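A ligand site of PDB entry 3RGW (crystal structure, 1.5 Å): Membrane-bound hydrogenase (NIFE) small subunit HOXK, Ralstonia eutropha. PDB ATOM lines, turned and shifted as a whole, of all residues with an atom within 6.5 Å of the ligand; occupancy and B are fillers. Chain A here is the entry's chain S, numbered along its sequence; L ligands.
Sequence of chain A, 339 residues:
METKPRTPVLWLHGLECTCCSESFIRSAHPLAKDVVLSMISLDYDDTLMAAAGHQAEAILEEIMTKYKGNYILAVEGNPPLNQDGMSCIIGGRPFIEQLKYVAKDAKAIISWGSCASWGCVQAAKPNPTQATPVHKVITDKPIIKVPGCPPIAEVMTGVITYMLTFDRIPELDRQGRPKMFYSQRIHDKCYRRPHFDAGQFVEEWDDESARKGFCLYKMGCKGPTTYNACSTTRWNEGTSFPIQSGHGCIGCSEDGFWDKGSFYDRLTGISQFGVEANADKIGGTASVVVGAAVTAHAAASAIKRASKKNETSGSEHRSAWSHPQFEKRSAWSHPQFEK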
ATOM      1  N   ILE A 186      28.305 -31.128   7.898  1.00  0.00           N
ATOM      2  CA  ILE A 186      27.010 -31.701   8.259  1.00  0.00           C
ATOM      3  C   ILE A 186      25.883 -30.945   7.550  1.00  0.00           C
ATOM      4  O   ILE A 186      24.929 -31.539   7.045  1.00  0.00           O
ATOM      5  CB  ILE A 186      26.750 -31.627   9.785  1.00  0.00           C
ATOM      6  CG1 ILE A 186      27.928 -32.216  10.551  1.00  0.00           C
ATOM      7  CG2 ILE A 186      25.446 -32.336  10.146  1.00  0.00           C
ATOM      8  CD1 ILE A 186      28.112 -33.701  10.351  1.00  0.00           C
ATOM      9  N   HIS A 187      26.042 -29.628   7.490  1.00  0.00           N
ATOM     10  CA  HIS A 187      24.989 -28.715   7.035  1.00  0.00           C
ATOM     11  C   HIS A 187      24.761 -28.806   5.513  1.00  0.00           C
ATOM     12  O   HIS A 187      23.731 -28.371   5.002  1.00  0.00           O
ATOM     13  CB  HIS A 187      25.381 -27.277   7.429  1.00  0.00           C
ATOM     14  CG  HIS A 187      24.373 -26.245   7.056  1.00  0.00           C
ATOM     15  ND1 HIS A 187      23.207 -26.038   7.762  1.00  0.00           N
ATOM     16  CD2 HIS A 187      24.409 -25.261   6.119  1.00  0.00           C
ATOM     17  CE1 HIS A 187      22.552 -25.019   7.250  1.00  0.00           C
ATOM     18  NE2 HIS A 187      23.261 -24.530   6.251  1.00  0.00           N
ATOM     19  N   ASP A 188      25.717 -29.399   4.796  1.00  0.00           N
ATOM     20  CA  ASP A 188      25.623 -29.498   3.333  1.00  0.00           C
ATOM     21  C   ASP A 188      24.455 -30.374   2.907  1.00  0.00           C
ATOM     22  O   ASP A 188      23.714 -30.029   1.983  1.00  0.00           O
ATOM     23  CB  ASP A 188      26.929 -30.048   2.748  1.00  0.00           C
ATOM     24  CG  ASP A 188      28.075 -29.066   2.858  1.00  0.00           C
ATOM     25  OD1 ASP A 188      27.812 -27.855   3.002  1.00  0.00           O
ATOM     26  OD2 ASP A 188      29.247 -29.514   2.790  1.00  0.00           O
ATOM     27  N   CYS A 190      22.398 -32.125   5.376  1.00  0.00           N
ATOM     28  CA  CYS A 190      21.453 -32.306   6.464  1.00  0.00           C
ATOM     29  C   CYS A 190      20.016 -32.265   5.958  1.00  0.00           C
ATOM     30  O   CYS A 190      19.631 -31.356   5.216  1.00  0.00           O
ATOM     31  CB  CYS A 190      21.645 -31.239   7.532  1.00  0.00           C
ATOM     32  SG  CYS A 190      20.493 -31.347   8.907  1.00  0.00           S
ATOM     33  N   TYR A 191      19.207 -33.249   6.376  1.00  0.00           N
ATOM     34  CA  TYR A 191      17.840 -33.378   5.873  1.00  0.00           C
ATOM     35  C   TYR A 191      16.936 -32.231   6.346  1.00  0.00           C
ATOM     36  O   TYR A 191      15.859 -32.027   5.800  1.00  0.00           O
ATOM     37  CB  TYR A 191      17.236 -34.739   6.267  1.00  0.00           C
ATOM     38  CG  TYR A 191      16.760 -34.792   7.694  1.00  0.00           C
ATOM     39  CD1 TYR A 191      17.664 -34.957   8.751  1.00  0.00           C
ATOM     40  CD2 TYR A 191      15.417 -34.656   8.007  1.00  0.00           C
ATOM     41  CE1 TYR A 191      17.230 -34.993  10.064  1.00  0.00           C
ATOM     42  CE2 TYR A 191      14.978 -34.680   9.313  1.00  0.00           C
ATOM     43  CZ  TYR A 191      15.879 -34.846  10.342  1.00  0.00           C
ATOM     44  OH  TYR A 191      15.449 -34.863  11.639  1.00  0.00           O
ATOM     45  N   ARG A 192      17.374 -31.504   7.368  1.00  0.00           N
ATOM     46  CA  ARG A 192      16.603 -30.347   7.856  1.00  0.00           C
ATOM     47  C   ARG A 192      16.916 -29.083   7.073  1.00  0.00           C
ATOM     48  O   ARG A 192      16.390 -28.014   7.370  1.00  0.00           O
ATOM     49  CB  ARG A 192      16.835 -30.123   9.351  1.00  0.00           C
ATOM     50  CG  ARG A 192      16.493 -31.329  10.208  1.00  0.00           C
ATOM     51  CD  ARG A 192      16.254 -30.929  11.682  1.00  0.00           C
ATOM     52  NE  ARG A 192      15.931 -32.103  12.491  1.00  0.00           N
ATOM     53  CZ  ARG A 192      15.277 -32.067  13.663  1.00  0.00           C
ATOM     54  NH1 ARG A 192      14.877 -30.916  14.174  1.00  0.00           N
ATOM     55  NH2 ARG A 192      15.029 -33.196  14.309  1.00  0.00           N
ATOM     56  N   ARG A 193      17.784 -29.206   6.080  1.00  0.00           N
ATOM     57  CA  ARG A 193      18.249 -28.053   5.314  1.00  0.00           C
ATOM     58  C   ARG A 193      17.088 -27.248   4.680  1.00  0.00           C
ATOM     59  O   ARG A 193      17.145 -26.013   4.624  1.00  0.00           O
ATOM     60  CB  ARG A 193      19.259 -28.483   4.254  1.00  0.00           C
ATOM     61  CG  ARG A 193      19.907 -27.336   3.518  1.00  0.00           C
ATOM     62  CD  ARG A 193      20.764 -26.492   4.443  1.00  0.00           C
ATOM     63  NE  ARG A 193      21.256 -25.299   3.772  1.00  0.00           N
ATOM     64  CZ  ARG A 193      22.398 -25.241   3.102  1.00  0.00           C
ATOM     65  NH1 ARG A 193      23.192 -26.303   3.044  1.00  0.00           N
ATOM     66  NH2 ARG A 193      22.756 -24.113   2.497  1.00  0.00           N
ATOM     67  N   PRO A 194      16.055 -27.942   4.176  1.00  0.00           N
ATOM     68  CA  PRO A 194      14.942 -27.212   3.587  1.00  0.00           C
ATOM     69  C   PRO A 194      14.275 -26.267   4.583  1.00  0.00           C
ATOM     70  O   PRO A 194      13.760 -25.221   4.199  1.00  0.00           O
ATOM     71  CB  PRO A 194      13.977 -28.326   3.154  1.00  0.00           C
ATOM     72  CG  PRO A 194      14.861 -29.471   2.855  1.00  0.00           C
ATOM     73  CD  PRO A 194      16.010 -29.384   3.851  1.00  0.00           C
ATOM     74  N   HIS A 195      14.315 -26.622   5.864  1.00  0.00           N
ATOM     75  CA  HIS A 195      13.771 -25.756   6.909  1.00  0.00           C
ATOM     76  C   HIS A 195      14.685 -24.567   7.168  1.00  0.00           C
ATOM     77  O   HIS A 195      14.231 -23.433   7.280  1.00  0.00           O
ATOM     78  CB  HIS A 195      13.521 -26.541   8.201  1.00  0.00           C
ATOM     79  CG  HIS A 195      12.426 -27.563   8.077  1.00  0.00           C
ATOM     80  ND1 HIS A 195      11.151 -27.236   7.693  1.00  0.00           N
ATOM     81  CD2 HIS A 195      12.439 -28.902   8.290  1.00  0.00           C
ATOM     82  CE1 HIS A 195      10.408 -28.334   7.676  1.00  0.00           C
ATOM     83  NE2 HIS A 195      11.168 -29.359   8.036  1.00  0.00           N
ATOM     84  N   PHE A 196      15.993 -24.827   7.237  1.00  0.00           N
ATOM     85  CA  PHE A 196      16.973 -23.766   7.370  1.00  0.00           C
ATOM     86  C   PHE A 196      16.796 -22.738   6.255  1.00  0.00           C
ATOM     87  O   PHE A 196      16.758 -21.529   6.509  1.00  0.00           O
ATOM     88  CB  PHE A 196      18.390 -24.325   7.334  1.00  0.00           C
ATOM     89  CG  PHE A 196      19.467 -23.273   7.373  1.00  0.00           C
ATOM     90  CD1 PHE A 196      20.001 -22.847   8.586  1.00  0.00           C
ATOM     91  CD2 PHE A 196      19.943 -22.711   6.199  1.00  0.00           C
ATOM     92  CE1 PHE A 196      21.000 -21.886   8.612  1.00  0.00           C
ATOM     93  CE2 PHE A 196      20.929 -21.746   6.227  1.00  0.00           C
ATOM     94  CZ  PHE A 196      21.465 -21.331   7.432  1.00  0.00           C
ATOM     95  N   PHE A 201      12.745 -22.609  12.191  1.00  0.00           N
ATOM     96  CA  PHE A 201      13.669 -22.990  13.268  1.00  0.00           C
ATOM     97  C   PHE A 201      12.941 -23.397  14.532  1.00  0.00           C
ATOM     98  O   PHE A 201      11.906 -22.821  14.882  1.00  0.00           O
ATOM     99  CB  PHE A 201      14.619 -21.829  13.587  1.00  0.00           C
ATOM    100  CG  PHE A 201      15.425 -21.364  12.424  1.00  0.00           C
ATOM    101  CD1 PHE A 201      16.535 -22.067  12.003  1.00  0.00           C
ATOM    102  CD2 PHE A 201      15.099 -20.183  11.762  1.00  0.00           C
ATOM    103  CE1 PHE A 201      17.301 -21.624  10.932  1.00  0.00           C
ATOM    104  CE2 PHE A 201      15.852 -19.735  10.693  1.00  0.00           C
ATOM    105  CZ  PHE A 201      16.964 -20.459  10.280  1.00  0.00           C
ATOM    106  N   PHE A 214      11.960 -28.980  12.532  1.00  0.00           N
ATOM    107  CA  PHE A 214      12.553 -27.745  11.994  1.00  0.00           C
ATOM    108  C   PHE A 214      14.051 -27.665  12.314  1.00  0.00           C
ATOM    109  O   PHE A 214      14.566 -28.407  13.145  1.00  0.00           O
ATOM    110  CB  PHE A 214      11.828 -26.511  12.565  1.00  0.00           C
ATOM    111  CG  PHE A 214      10.539 -26.178  11.853  1.00  0.00           C
ATOM    112  CD1 PHE A 214       9.946 -27.093  10.998  1.00  0.00           C
ATOM    113  CD2 PHE A 214       9.917 -24.958  12.059  1.00  0.00           C
ATOM    114  CE1 PHE A 214       8.761 -26.788  10.343  1.00  0.00           C
ATOM    115  CE2 PHE A 214       8.726 -24.651  11.412  1.00  0.00           C
ATOM    116  CZ  PHE A 214       8.147 -25.571  10.555  1.00  0.00           C
ATOM    117  N   CYS A 215      14.739 -26.770  11.624  1.00  0.00           N
ATOM    118  CA  CYS A 215      16.194 -26.629  11.756  1.00  0.00           C
ATOM    119  C   CYS A 215      16.596 -26.277  13.177  1.00  0.00           C
ATOM    120  O   CYS A 215      15.867 -25.570  13.891  1.00  0.00           O
ATOM    121  CB  CYS A 215      16.709 -25.576  10.779  1.00  0.00           C
ATOM    122  SG  CYS A 215      18.428 -25.135  10.987  1.00  0.00           S
ATOM    123  N   LEU A 216      17.768 -26.767  13.605  1.00  0.00           N
ATOM    124  CA  LEU A 216      18.226 -26.628  14.983  1.00  0.00           C
ATOM    125  C   LEU A 216      19.298 -25.532  15.143  1.00  0.00           C
ATOM    126  O   LEU A 216      19.919 -25.402  16.196  1.00  0.00           O
ATOM    127  CB  LEU A 216      18.756 -27.973  15.512  1.00  0.00           C
ATOM    128  CG  LEU A 216      17.697 -29.072  15.614  1.00  0.00           C
ATOM    129  CD1 LEU A 216      18.342 -30.444  15.791  1.00  0.00           C
ATOM    130  CD2 LEU A 216      16.716 -28.783  16.740  1.00  0.00           C
ATOM    131  N   TYR A 217      19.478 -24.722  14.097  1.00  0.00           N
ATOM    132  CA  TYR A 217      20.496 -23.654  14.102  1.00  0.00           C
ATOM    133  C   TYR A 217      20.368 -22.750  15.340  1.00  0.00           C
ATOM    134  O   TYR A 217      21.362 -22.401  15.977  1.00  0.00           O
ATOM    135  CB  TYR A 217      20.392 -22.811  12.834  1.00  0.00           C
ATOM    136  CG  TYR A 217      21.458 -21.749  12.710  1.00  0.00           C
ATOM    137  CD1 TYR A 217      22.624 -21.999  12.005  1.00  0.00           C
ATOM    138  CD2 TYR A 217      21.290 -20.500  13.289  1.00  0.00           C
ATOM    139  CE1 TYR A 217      23.606 -21.025  11.876  1.00  0.00           C
ATOM    140  CE2 TYR A 217      22.262 -19.512  13.161  1.00  0.00           C
ATOM    141  CZ  TYR A 217      23.411 -19.788  12.453  1.00  0.00           C
ATOM    142  OH  TYR A 217      24.385 -18.813  12.318  1.00  0.00           O
ATOM    143  N   LYS A 218      19.144 -22.358  15.654  1.00  0.00           N
ATOM    144  CA  LYS A 218      18.921 -21.405  16.732  1.00  0.00           C
ATOM    145  C   LYS A 218      18.999 -22.060  18.112  1.00  0.00           C
ATOM    146  O   LYS A 218      18.999 -21.377  19.131  1.00  0.00           O
ATOM    147  CB  LYS A 218      17.602 -20.666  16.539  1.00  0.00           C
ATOM    148  CG  LYS A 218      17.593 -19.779  15.297  1.00  0.00           C
ATOM    149  CD  LYS A 218      16.350 -18.929  15.210  1.00  0.00           C
ATOM    150  CE  LYS A 218      16.456 -17.957  14.048  1.00  0.00           C
ATOM    151  NZ  LYS A 218      15.272 -17.077  13.929  1.00  0.00           N
ATOM    152  N   CYS A 221      23.046 -25.544  16.900  1.00  0.00           N
ATOM    153  CA  CYS A 221      23.613 -26.524  15.971  1.00  0.00           C
ATOM    154  C   CYS A 221      24.885 -26.001  15.307  1.00  0.00           C
ATOM    155  O   CYS A 221      24.882 -24.933  14.694  1.00  0.00           O
ATOM    156  CB  CYS A 221      22.604 -26.939  14.902  1.00  0.00           C
ATOM    157  SG  CYS A 221      23.225 -28.259  13.792  1.00  0.00           S
ATOM    158  N   LYS A 222      25.949 -26.781  15.397  1.00  0.00           N
ATOM    159  CA  LYS A 222      27.231 -26.392  14.808  1.00  0.00           C
ATOM    160  C   LYS A 222      27.485 -27.134  13.481  1.00  0.00           C
ATOM    161  O   LYS A 222      28.595 -27.116  12.954  1.00  0.00           O
ATOM    162  CB  LYS A 222      28.375 -26.643  15.796  1.00  0.00           C
ATOM    163  CG  LYS A 222      28.274 -25.818  17.090  1.00  0.00           C
ATOM    164  CD  LYS A 222      27.925 -24.365  16.780  1.00  0.00           C
ATOM    165  CE  LYS A 222      28.034 -23.476  18.025  1.00  0.00           C
ATOM    166  NZ  LYS A 222      27.093 -23.870  19.121  1.00  0.00           N
ATOM    167  N   GLY A 223      26.432 -27.711  12.926  1.00  0.00           N
ATOM    168  CA  GLY A 223      26.522 -28.373  11.635  1.00  0.00           C
ATOM    169  C   GLY A 223      27.168 -27.531  10.553  1.00  0.00           C
ATOM    170  O   GLY A 223      27.910 -28.042   9.722  1.00  0.00           O
ATOM    171  N   PRO A 224      26.872 -26.218  10.540  1.00  0.00           N
ATOM    172  CA  PRO A 224      27.345 -25.372   9.449  1.00  0.00           C
ATOM    173  C   PRO A 224      28.872 -25.183   9.438  1.00  0.00           C
ATOM    174  O   PRO A 224      29.419 -24.724   8.436  1.00  0.00           O
ATOM    175  CB  PRO A 224      26.637 -24.046   9.699  1.00  0.00           C
ATOM    176  CG  PRO A 224      25.392 -24.416  10.396  1.00  0.00           C
ATOM    177  CD  PRO A 224      25.784 -25.567  11.296  1.00  0.00           C
ATOM    178  N   PHE A 241      21.312 -39.776  13.419  1.00  0.00           N
ATOM    179  CA  PHE A 241      22.441 -38.980  13.869  1.00  0.00           C
ATOM    180  C   PHE A 241      21.928 -37.865  14.742  1.00  0.00           C
ATOM    181  O   PHE A 241      20.722 -37.704  14.890  1.00  0.00           O
ATOM    182  CB  PHE A 241      23.270 -38.453  12.664  1.00  0.00           C
ATOM    183  CG  PHE A 241      22.577 -37.363  11.861  1.00  0.00           C
ATOM    184  CD1 PHE A 241      21.416 -37.634  11.132  1.00  0.00           C
ATOM    185  CD2 PHE A 241      23.157 -36.108  11.725  1.00  0.00           C
ATOM    186  CE1 PHE A 241      20.825 -36.650  10.347  1.00  0.00           C
ATOM    187  CE2 PHE A 241      22.565 -35.125  10.940  1.00  0.00           C
ATOM    188  CZ  PHE A 241      21.395 -35.399  10.255  1.00  0.00           C
ATOM    189  N   ILE A 243      21.267 -34.779  14.860  1.00  0.00           N
ATOM    190  CA  ILE A 243      20.241 -33.853  14.408  1.00  0.00           C
ATOM    191  C   ILE A 243      18.907 -34.575  14.145  1.00  0.00           C
ATOM    192  O   ILE A 243      17.831 -34.070  14.489  1.00  0.00           O
ATOM    193  CB  ILE A 243      20.689 -33.099  13.152  1.00  0.00           C
ATOM    194  CG1 ILE A 243      21.741 -32.061  13.532  1.00  0.00           C
ATOM    195  CG2 ILE A 243      19.495 -32.434  12.464  1.00  0.00           C
ATOM    196  CD1 ILE A 243      22.743 -31.773  12.425  1.00  0.00           C
ATOM    197  N   GLY A 248      21.133 -30.477  18.260  1.00  0.00           N
ATOM    198  CA  GLY A 248      22.088 -29.872  17.333  1.00  0.00           C
ATOM    199  C   GLY A 248      23.432 -30.590  17.385  1.00  0.00           C
ATOM    200  O   GLY A 248      23.833 -31.129  18.411  1.00  0.00           O
ATOM    201  N   CYS A 249      24.127 -30.593  16.256  1.00  0.00           N
ATOM    202  CA  CYS A 249      25.536 -30.937  16.234  1.00  0.00           C
ATOM    203  C   CYS A 249      26.282 -30.059  17.247  1.00  0.00           C
ATOM    204  O   CYS A 249      26.011 -28.871  17.343  1.00  0.00           O
ATOM    205  CB  CYS A 249      26.090 -30.708  14.817  1.00  0.00           C
ATOM    206  SG  CYS A 249      27.870 -30.979  14.614  1.00  0.00           S
HETATM  207 FE1  LIG L   1      20.853 -29.250   9.824  1.00  0.00          FE
HETATM  208 FE2  LIG L   1      19.916 -26.842  10.562  1.00  0.00          FE
HETATM  209 FE3  LIG L   1      22.060 -27.918  11.837  1.00  0.00          FE
HETATM  210 FE4  LIG L   1      22.278 -27.065   9.274  1.00  0.00          FE
HETATM  211  S1  LIG L   1      21.857 -25.767  11.113  1.00  0.00           S
HETATM  212  S2  LIG L   1      23.121 -28.988  10.071  1.00  0.00           S
HETATM  213  S3  LIG L   1      20.209 -27.596   8.406  1.00  0.00           S
HETATM  214  S4  LIG L   1      19.902 -28.758  11.803  1.00  0.00           S
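An iron atom (FE4) of the ligand is bound by a ring nitrogen (ND1) of His 187 (2.1 Å). FE3 of the ligand is bound by SG of Cys 221, 2.3 Å away. An iron atom (FE2) of the ligand is bound by the side-chain sulfur of Cys 215, 2.3 Å away. FE1 of the ligand is bound by SG of Cys 190 (2.3 Å). A sulfur (S4) of the ligand sits close to the backbone NH (N) of Leu 216, 3.4 Å away. The backbone NH (N) of Arg 193 sits close to a sulfur (S3) of the ligand, 3.7 Å away.
The backbone carbonyl oxygen (O) of His 187 is in hydrogen-bond range of the guanidinium group (NH1) of Arg 193 (2.9 Å). The backbone carbonyl oxygen (O) of Gly 223 lies within hydrogen-bond range of the backbone NH (N) of His 187. The backbone carbonyl oxygen (O) of Leu 216 sits at hydrogen-bond distance from the backbone NH (N) of Cys 221, at 3.2 Å. The side-chain sulfur of Cys 221 sits close to the backbone NH of Gly 223, at 3.4 Å. N of Cys 249 sits close to SG of Cys 221. SG of Cys 190 lies close to N of Arg 192 (3.5 Å). NH2 of Arg 192 is in hydrogen-bond range of O of Ile 243, 2.9 Å away. The guanidinium group of Arg 192 is in hydrogen-bond range of the backbone carbonyl oxygen of Phe 214 (2.7 Å).
Merely in contact with the ligand: Arg 192, Phe 196, Tyr 217, Gly 223, Pro 224 and Ile 243. Hydrophobic or aromatic side chains that line the ligand: His 187, Phe 196, Leu 216, Tyr 217, Pro 224 and Ile 243. Within 4 Å of the ligand: His 187, Cys 190, Arg 192, Arg 193, Phe 196, Cys 215, Leu 216, Tyr 217, Cys 221, Gly 223, Pro 224 and Ile 243. Along chain A the residues within 4 Å of the ligand span positions 187 to 243. The nearest printed residue that does not touch the ligand is Ile 186 (4.1 Å).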
